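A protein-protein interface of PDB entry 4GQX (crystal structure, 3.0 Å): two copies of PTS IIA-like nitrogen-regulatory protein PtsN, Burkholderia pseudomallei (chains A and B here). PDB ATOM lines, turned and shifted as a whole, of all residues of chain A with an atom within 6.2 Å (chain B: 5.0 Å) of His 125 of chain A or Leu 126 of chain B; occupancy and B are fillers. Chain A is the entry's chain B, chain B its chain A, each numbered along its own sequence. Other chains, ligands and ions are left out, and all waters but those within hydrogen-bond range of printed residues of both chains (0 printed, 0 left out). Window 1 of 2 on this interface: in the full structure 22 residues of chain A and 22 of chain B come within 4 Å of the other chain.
Among the printed residues, merely in contact across the chains: His 79 of chain A with Glu 127 of chain B, Leu 129 of chain A with Ser 130 of chain B, Leu 126 of chain A with His 125 of chain B, Ser 130 of chain A with Leu 129 of chain B, His 125 of chain A with Leu 126 of chain B, His 79 of chain A with Leu 126 of chain B, Arg 81 of chain A with Gln 123 of chain B, Ala 121 of chain A with Gln 123 of chain B, Ala 121 of chain A with Thr 122 of chain B, Leu 129 of chain A with Leu 126 of chain B, Leu 126 of chain A with Leu 129 of chain B and Leu 129 of chain A with Leu 129 of chain B.
OG1 of Thr 122 of chain B lies close to ND1 of His 125 of chain B.
OG of Ser 130 of chain B lies close to O of Leu 126 of chain B.
The backbone carbonyl oxygen of Glu 127 of chain B is in hydrogen-bond range of the side-chain hydroxyl of Ser 130 of chain B (3.3 Å).
NH1 of Arg 81 of chain A is in hydrogen-bond range of O of Glu 119 of chain A, at 3.2 Å.
OG1 of Thr 122 of chain A lies close to ND1 of His 125 of chain A (3.4 Å).
The backbone carbonyl oxygen of Leu 126 of chain A sits close to the side-chain hydroxyl of Ser 130 of chain A (3.5 Å).
Of chain B, only Leu 126 comes within 4 Å of His 125 of chain A.
Printed residues of chain A within 4 Å of Ser 130 of chain B: Leu 129.
Of the printed residues of chain B, Leu 126 of chain A touches His 125 (3.4 Å) and Leu 129 (3.8 Å).
Printed residues of chain B within 4 Å of Glu 119 of chain A: Gln 123 (3.2 Å).
Printed residues of chain A within 4 Å of Glu 127 of chain B: His 79.
Of the printed residues of chain B, Ser 130 of chain A touches Leu 129.
Ala 124 of chain A touches none of the printed residues of chain B.
The nearest printed residue of chain B that does not touch Ser 130 of chain A is Leu 126 of chain B (6.6 Å).
O of Glu 119 of chain A sits at hydrogen-bond distance from NE2 of Gln 123 of chain B, 3.2 Å away.
Hydrophobic or aromatic side chains of chain B that line the printed part of chain A: His 125, Leu 126 and Leu 129.
Along chain B the printed residues that touch a printed residue of chain A span positions 122 to 130.
Hydrophobic or aromatic side chains of chain A within 4 Å of the printed part of chain B: His 79, Ala 121, His 125, Leu 126 and Leu 129.
Among the printed residues, 13 pairs touch across the chains.
Among the printed residues, no Asp or Glu carboxylate lies within 4 Å of a Lys or Arg side-chain nitrogen of the other chain.
His 125 of chain A touches Leu 126 of chain B, and with the chains exchanged Leu 126 of chain A touches His 125 of chain B.
Leu 126 of chain A touches Leu 129 of chain B, and with the chains exchanged Leu 129 of chain A touches Leu 126 of chain B.
Leu 129 of chain A touches its own counterpart, Leu 129 of chain B.
Leu 129 of chain A touches Ser 130 of chain B, and with the chains exchanged Ser 130 of chain A touches Leu 129 of chain B.
Of the 13 pairs that touch across the chains among the printed residues, 7 have their exchanged pair printed and touching as well.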
ATOM      1  N   HIS A  79      -5.196  13.868  23.060  1.00  0.00           N
ATOM      2  CA  HIS A  79      -4.003  14.585  22.601  1.00  0.00           C
ATOM      3  C   HIS A  79      -4.013  14.693  21.089  1.00  0.00           C
ATOM      4  O   HIS A  79      -4.884  14.110  20.435  1.00  0.00           O
ATOM      5  CB  HIS A  79      -2.740  13.860  23.044  1.00  0.00           C
ATOM      6  CG  HIS A  79      -2.717  12.415  22.654  1.00  0.00           C
ATOM      7  ND1 HIS A  79      -2.169  11.973  21.472  1.00  0.00           N
ATOM      8  CD2 HIS A  79      -3.193  11.314  23.284  1.00  0.00           C
ATOM      9  CE1 HIS A  79      -2.298  10.661  21.396  1.00  0.00           C
ATOM     10  NE2 HIS A  79      -2.919  10.237  22.482  1.00  0.00           N
ATOM     11  N   ARG A  81      -1.695  16.839  17.375  1.00  0.00           N
ATOM     12  CA  ARG A  81      -0.629  17.668  16.843  1.00  0.00           C
ATOM     13  C   ARG A  81      -1.256  19.035  16.575  1.00  0.00           C
ATOM     14  O   ARG A  81      -2.446  19.119  16.281  1.00  0.00           O
ATOM     15  CB  ARG A  81      -0.064  17.066  15.533  1.00  0.00           C
ATOM     16  CG  ARG A  81       0.513  15.619  15.622  1.00  0.00           C
ATOM     17  CD  ARG A  81       2.049  15.592  15.708  1.00  0.00           C
ATOM     18  NE  ARG A  81       2.547  14.588  16.661  1.00  0.00           N
ATOM     19  CZ  ARG A  81       3.800  14.524  17.130  1.00  0.00           C
ATOM     20  NH1 ARG A  81       4.718  15.407  16.722  1.00  0.00           N
ATOM     21  NH2 ARG A  81       4.135  13.580  18.017  1.00  0.00           N
ATOM     22  N   PRO A  88       5.244  21.861  23.468  1.00  0.00           N
ATOM     23  CA  PRO A  88       3.990  21.171  23.793  1.00  0.00           C
ATOM     24  C   PRO A  88       3.180  21.909  24.853  1.00  0.00           C
ATOM     25  O   PRO A  88       3.723  22.788  25.543  1.00  0.00           O
ATOM     26  CB  PRO A  88       4.458  19.818  24.351  1.00  0.00           C
ATOM     27  CG  PRO A  88       5.912  19.971  24.630  1.00  0.00           C
ATOM     28  CD  PRO A  88       6.401  20.965  23.626  1.00  0.00           C
ATOM     29  N   LEU A 115      -3.004  16.588  26.100  1.00  0.00           N
ATOM     30  CA  LEU A 115      -1.671  16.911  25.609  1.00  0.00           C
ATOM     31  C   LEU A 115      -1.670  17.362  24.158  1.00  0.00           C
ATOM     32  O   LEU A 115      -2.105  16.596  23.289  1.00  0.00           O
ATOM     33  CB  LEU A 115      -0.731  15.701  25.765  1.00  0.00           C
ATOM     34  CG  LEU A 115       0.706  15.941  25.250  1.00  0.00           C
ATOM     35  CD1 LEU A 115       1.434  16.965  26.079  1.00  0.00           C
ATOM     36  CD2 LEU A 115       1.515  14.669  25.203  1.00  0.00           C
ATOM     37  N   VAL A 117       0.982  18.609  21.108  1.00  0.00           N
ATOM     38  CA  VAL A 117       2.390  18.693  20.691  1.00  0.00           C
ATOM     39  C   VAL A 117       2.581  19.310  19.294  1.00  0.00           C
ATOM     40  O   VAL A 117       1.696  19.223  18.428  1.00  0.00           O
ATOM     41  CB  VAL A 117       3.060  17.312  20.672  1.00  0.00           C
ATOM     42  CG1 VAL A 117       3.352  16.827  22.090  1.00  0.00           C
ATOM     43  CG2 VAL A 117       2.232  16.311  19.839  1.00  0.00           C
ATOM     44  N   PRO A 118       3.750  19.924  19.058  1.00  0.00           N
ATOM     45  CA  PRO A 118       3.956  20.481  17.747  1.00  0.00           C
ATOM     46  C   PRO A 118       4.078  19.382  16.682  1.00  0.00           C
ATOM     47  O   PRO A 118       4.347  18.223  17.012  1.00  0.00           O
ATOM     48  CB  PRO A 118       5.245  21.308  17.907  1.00  0.00           C
ATOM     49  CG  PRO A 118       5.890  20.837  19.136  1.00  0.00           C
ATOM     50  CD  PRO A 118       4.809  20.319  20.004  1.00  0.00           C
ATOM     51  N   GLU A 119       3.838  19.759  15.426  1.00  0.00           N
ATOM     52  CA  GLU A 119       3.933  18.864  14.290  1.00  0.00           C
ATOM     53  C   GLU A 119       5.286  18.202  14.279  1.00  0.00           C
ATOM     54  O   GLU A 119       5.396  17.003  14.033  1.00  0.00           O
ATOM     55  CB  GLU A 119       3.778  19.664  12.998  1.00  0.00           C
ATOM     56  CG  GLU A 119       2.411  20.324  12.803  1.00  0.00           C
ATOM     57  CD  GLU A 119       1.349  19.351  12.285  1.00  0.00           C
ATOM     58  OE1 GLU A 119       1.228  18.221  12.848  1.00  0.00           O
ATOM     59  OE2 GLU A 119       0.635  19.729  11.317  1.00  0.00           O
ATOM     60  N   GLN A 120       6.307  19.013  14.545  1.00  0.00           N
ATOM     61  CA  GLN A 120       7.676  18.572  14.589  1.00  0.00           C
ATOM     62  C   GLN A 120       7.923  17.783  15.869  1.00  0.00           C
ATOM     63  O   GLN A 120       7.964  18.359  16.960  1.00  0.00           O
ATOM     64  CB  GLN A 120       8.604  19.782  14.498  1.00  0.00           C
ATOM     65  CG  GLN A 120      10.102  19.466  14.608  1.00  0.00           C
ATOM     66  CD  GLN A 120      10.621  18.544  13.511  1.00  0.00           C
ATOM     67  OE1 GLN A 120      10.341  17.343  13.491  1.00  0.00           O
ATOM     68  NE2 GLN A 120      11.410  19.108  12.607  1.00  0.00           N
ATOM     69  N   ALA A 121       8.101  16.466  15.698  1.00  0.00           N
ATOM     70  CA  ALA A 121       8.208  15.495  16.771  1.00  0.00           C
ATOM     71  C   ALA A 121       9.541  15.576  17.478  1.00  0.00           C
ATOM     72  O   ALA A 121      10.557  15.784  16.853  1.00  0.00           O
ATOM     73  CB  ALA A 121       8.002  14.112  16.217  1.00  0.00           C
ATOM     74  N   THR A 122       9.508  15.420  18.796  1.00  0.00           N
ATOM     75  CA  THR A 122      10.680  15.374  19.650  1.00  0.00           C
ATOM     76  C   THR A 122      10.702  14.005  20.261  1.00  0.00           C
ATOM     77  O   THR A 122       9.647  13.413  20.556  1.00  0.00           O
ATOM     78  CB  THR A 122      10.543  16.307  20.891  1.00  0.00           C
ATOM     79  OG1 THR A 122       9.932  17.543  20.522  1.00  0.00           O
ATOM     80  CG2 THR A 122      11.901  16.588  21.600  1.00  0.00           C
ATOM     81  N   GLN A 123      11.912  13.536  20.514  1.00  0.00           N
ATOM     82  CA  GLN A 123      12.161  12.404  21.393  1.00  0.00           C
ATOM     83  C   GLN A 123      11.405  12.499  22.751  1.00  0.00           C
ATOM     84  O   GLN A 123      10.983  11.490  23.310  1.00  0.00           O
ATOM     85  CB  GLN A 123      13.670  12.264  21.604  1.00  0.00           C
ATOM     86  CG  GLN A 123      14.520  12.181  20.289  1.00  0.00           C
ATOM     87  CD  GLN A 123      14.560  13.503  19.403  1.00  0.00           C
ATOM     88  OE1 GLN A 123      14.152  14.599  19.842  1.00  0.00           O
ATOM     89  NE2 GLN A 123      15.058  13.368  18.152  1.00  0.00           N
ATOM     90  N   ALA A 124      11.231  13.720  23.252  1.00  0.00           N
ATOM     91  CA  ALA A 124      10.549  13.984  24.530  1.00  0.00           C
ATOM     92  C   ALA A 124       9.065  13.691  24.503  1.00  0.00           C
ATOM     93  O   ALA A 124       8.489  13.356  25.530  1.00  0.00           O
ATOM     94  CB  ALA A 124      10.765  15.428  24.962  1.00  0.00           C
ATOM     95  N   HIS A 125       8.444  13.824  23.336  1.00  0.00           N
ATOM     96  CA  HIS A 125       7.002  13.665  23.205  1.00  0.00           C
ATOM     97  C   HIS A 125       6.560  12.319  23.754  1.00  0.00           C
ATOM     98  O   HIS A 125       5.615  12.244  24.508  1.00  0.00           O
ATOM     99  CB  HIS A 125       6.594  13.818  21.744  1.00  0.00           C
ATOM    100  CG  HIS A 125       6.679  15.228  21.227  1.00  0.00           C
ATOM    101  ND1 HIS A 125       7.184  16.275  21.968  1.00  0.00           N
ATOM    102  CD2 HIS A 125       6.333  15.755  20.027  1.00  0.00           C
ATOM    103  CE1 HIS A 125       7.119  17.391  21.262  1.00  0.00           C
ATOM    104  NE2 HIS A 125       6.615  17.100  20.077  1.00  0.00           N
ATOM    105  N   LEU A 126       7.285  11.268  23.399  1.00  0.00           N
ATOM    106  CA  LEU A 126       6.994   9.933  23.858  1.00  0.00           C
ATOM    107  C   LEU A 126       7.063   9.821  25.367  1.00  0.00           C
ATOM    108  O   LEU A 126       6.183   9.211  25.989  1.00  0.00           O
ATOM    109  CB  LEU A 126       7.975   8.956  23.244  1.00  0.00           C
ATOM    110  CG  LEU A 126       7.675   7.490  23.529  1.00  0.00           C
ATOM    111  CD1 LEU A 126       7.932   6.601  22.315  1.00  0.00           C
ATOM    112  CD2 LEU A 126       8.454   7.015  24.739  1.00  0.00           C
ATOM    113  N   GLU A 127       8.117  10.398  25.949  1.00  0.00           N
ATOM    114  CA  GLU A 127       8.403  10.279  27.391  1.00  0.00           C
ATOM    115  C   GLU A 127       7.470  11.167  28.226  1.00  0.00           C
ATOM    116  O   GLU A 127       7.278  10.945  29.436  1.00  0.00           O
ATOM    117  CB  GLU A 127       9.866  10.609  27.690  1.00  0.00           C
ATOM    118  CG  GLU A 127      10.866   9.986  26.725  1.00  0.00           C
ATOM    119  CD  GLU A 127      11.203   8.522  27.048  1.00  0.00           C
ATOM    120  OE1 GLU A 127      10.743   8.031  28.108  1.00  0.00           O
ATOM    121  OE2 GLU A 127      11.941   7.883  26.239  1.00  0.00           O
ATOM    122  N   ILE A 128       6.873  12.167  27.589  1.00  0.00           N
ATOM    123  CA  ILE A 128       5.974  13.029  28.329  1.00  0.00           C
ATOM    124  C   ILE A 128       4.548  12.475  28.349  1.00  0.00           C
ATOM    125  O   ILE A 128       3.880  12.498  29.375  1.00  0.00           O
ATOM    126  CB  ILE A 128       6.056  14.490  27.871  1.00  0.00           C
ATOM    127  CG1 ILE A 128       4.774  15.213  28.188  1.00  0.00           C
ATOM    128  CG2 ILE A 128       6.196  14.615  26.391  1.00  0.00           C
ATOM    129  CD1 ILE A 128       3.461  14.852  27.498  1.00  0.00           C
ATOM    130  N   LEU A 129       4.098  11.945  27.222  1.00  0.00           N
ATOM    131  CA  LEU A 129       2.867  11.162  27.169  1.00  0.00           C
ATOM    132  C   LEU A 129       2.971   9.938  28.058  1.00  0.00           C
ATOM    133  O   LEU A 129       1.981   9.528  28.666  1.00  0.00           O
ATOM    134  CB  LEU A 129       2.622  10.694  25.730  1.00  0.00           C
ATOM    135  CG  LEU A 129       1.373   9.912  25.267  1.00  0.00           C
ATOM    136  CD1 LEU A 129       1.437   8.464  25.637  1.00  0.00           C
ATOM    137  CD2 LEU A 129       0.061  10.508  25.725  1.00  0.00           C
ATOM    138  N   SER A 130       4.152   9.320  28.109  1.00  0.00           N
ATOM    139  CA  SER A 130       4.300   8.085  28.877  1.00  0.00           C
ATOM    140  C   SER A 130       4.263   8.383  30.365  1.00  0.00           C
ATOM    141  O   SER A 130       3.761   7.594  31.139  1.00  0.00           O
ATOM    142  CB  SER A 130       5.573   7.315  28.483  1.00  0.00           C
ATOM    143  OG  SER A 130       6.721   7.816  29.137  1.00  0.00           O
ATOM    144  N   THR B 122       9.513  10.130  15.342  1.00  0.00           N
ATOM    145  CA  THR B 122       8.337  10.179  14.477  1.00  0.00           C
ATOM    146  C   THR B 122       7.178  10.601  15.338  1.00  0.00           C
ATOM    147  O   THR B 122       7.108  10.256  16.532  1.00  0.00           O
ATOM    148  CB  THR B 122       7.913   8.769  13.961  1.00  0.00           C
ATOM    149  OG1 THR B 122       9.063   7.987  13.655  1.00  0.00           O
ATOM    150  CG2 THR B 122       6.996   8.833  12.711  1.00  0.00           C
ATOM    151  N   GLN B 123       6.244  11.301  14.707  1.00  0.00           N
ATOM    152  CA  GLN B 123       4.909  11.528  15.247  1.00  0.00           C
ATOM    153  C   GLN B 123       4.215  10.229  15.714  1.00  0.00           C
ATOM    154  O   GLN B 123       3.421  10.245  16.649  1.00  0.00           O
ATOM    155  CB  GLN B 123       4.062  12.226  14.192  1.00  0.00           C
ATOM    156  CG  GLN B 123       4.673  13.546  13.593  1.00  0.00           C
ATOM    157  CD  GLN B 123       5.976  13.364  12.723  1.00  0.00           C
ATOM    158  OE1 GLN B 123       6.355  12.241  12.334  1.00  0.00           O
ATOM    159  NE2 GLN B 123       6.650  14.493  12.430  1.00  0.00           N
ATOM    160  N   ALA B 124       4.534   9.112  15.065  1.00  0.00           N
ATOM    161  CA  ALA B 124       3.973   7.797  15.395  1.00  0.00           C
ATOM    162  C   ALA B 124       4.460   7.236  16.715  1.00  0.00           C
ATOM    163  O   ALA B 124       3.744   6.463  17.350  1.00  0.00           O
ATOM    164  CB  ALA B 124       4.281   6.802  14.290  1.00  0.00           C
ATOM    165  N   HIS B 125       5.674   7.604  17.114  1.00  0.00           N
ATOM    166  CA  HIS B 125       6.296   7.051  18.306  1.00  0.00           C
ATOM    167  C   HIS B 125       5.394   7.237  19.512  1.00  0.00           C
ATOM    168  O   HIS B 125       5.188   6.312  20.284  1.00  0.00           O
ATOM    169  CB  HIS B 125       7.642   7.721  18.541  1.00  0.00           C
ATOM    170  CG  HIS B 125       8.721   7.285  17.589  1.00  0.00           C
ATOM    171  ND1 HIS B 125       8.494   6.420  16.540  1.00  0.00           N
ATOM    172  CD2 HIS B 125      10.035   7.609  17.525  1.00  0.00           C
ATOM    173  CE1 HIS B 125       9.622   6.210  15.886  1.00  0.00           C
ATOM    174  NE2 HIS B 125      10.570   6.925  16.459  1.00  0.00           N
ATOM    175  N   LEU B 126       4.828   8.437  19.635  1.00  0.00           N
ATOM    176  CA  LEU B 126       3.922   8.764  20.716  1.00  0.00           C
ATOM    177  C   LEU B 126       2.690   7.885  20.708  1.00  0.00           C
ATOM    178  O   LEU B 126       2.275   7.406  21.758  1.00  0.00           O
ATOM    179  CB  LEU B 126       3.507  10.221  20.628  1.00  0.00           C
ATOM    180  CG  LEU B 126       2.674  10.699  21.823  1.00  0.00           C
ATOM    181  CD1 LEU B 126       3.027  12.128  22.249  1.00  0.00           C
ATOM    182  CD2 LEU B 126       1.179  10.557  21.546  1.00  0.00           C
ATOM    183  N   GLU B 127       2.108   7.685  19.525  1.00  0.00           N
ATOM    184  CA  GLU B 127       0.825   6.973  19.372  1.00  0.00           C
ATOM    185  C   GLU B 127       1.017   5.459  19.473  1.00  0.00           C
ATOM    186  O   GLU B 127       0.053   4.694  19.701  1.00  0.00           O
ATOM    187  CB  GLU B 127       0.135   7.321  18.057  1.00  0.00           C
ATOM    188  CG  GLU B 127       0.148   8.798  17.712  1.00  0.00           C
ATOM    189  CD  GLU B 127      -0.948   9.596  18.414  1.00  0.00           C
ATOM    190  OE1 GLU B 127      -1.830   8.966  19.044  1.00  0.00           O
ATOM    191  OE2 GLU B 127      -0.927  10.852  18.308  1.00  0.00           O
ATOM    192  N   ILE B 128       2.255   5.009  19.317  1.00  0.00           N
ATOM    193  CA  ILE B 128       2.487   3.584  19.444  1.00  0.00           C
ATOM    194  C   ILE B 128       2.761   3.208  20.893  1.00  0.00           C
ATOM    195  O   ILE B 128       2.264   2.215  21.374  1.00  0.00           O
ATOM    196  CB  ILE B 128       3.537   3.065  18.454  1.00  0.00           C
ATOM    197  CG1 ILE B 128       4.183   1.812  18.973  1.00  0.00           C
ATOM    198  CG2 ILE B 128       4.667   4.023  18.287  1.00  0.00           C
ATOM    199  CD1 ILE B 128       5.051   1.822  20.232  1.00  0.00           C
ATOM    200  N   LEU B 129       3.524   4.029  21.593  1.00  0.00           N
ATOM    201  CA  LEU B 129       3.706   3.878  23.036  1.00  0.00           C
ATOM    202  C   LEU B 129       2.386   4.070  23.756  1.00  0.00           C
ATOM    203  O   LEU B 129       2.141   3.443  24.789  1.00  0.00           O
ATOM    204  CB  LEU B 129       4.703   4.928  23.539  1.00  0.00           C
ATOM    205  CG  LEU B 129       5.167   5.095  24.998  1.00  0.00           C
ATOM    206  CD1 LEU B 129       4.088   5.716  25.837  1.00  0.00           C
ATOM    207  CD2 LEU B 129       5.654   3.817  25.641  1.00  0.00           C
ATOM    208  N   SER B 130       1.533   4.950  23.232  1.00  0.00           N
ATOM    209  CA  SER B 130       0.273   5.231  23.918  1.00  0.00           C
ATOM    210  C   SER B 130      -0.711   4.069  23.752  1.00  0.00           C
ATOM    211  O   SER B 130      -1.509   3.788  24.635  1.00  0.00           O
ATOM    212  CB  SER B 130      -0.337   6.563  23.454  1.00  0.00           C
ATOM    213  OG  SER B 130      -1.032   6.420  22.234  1.00  0.00           O
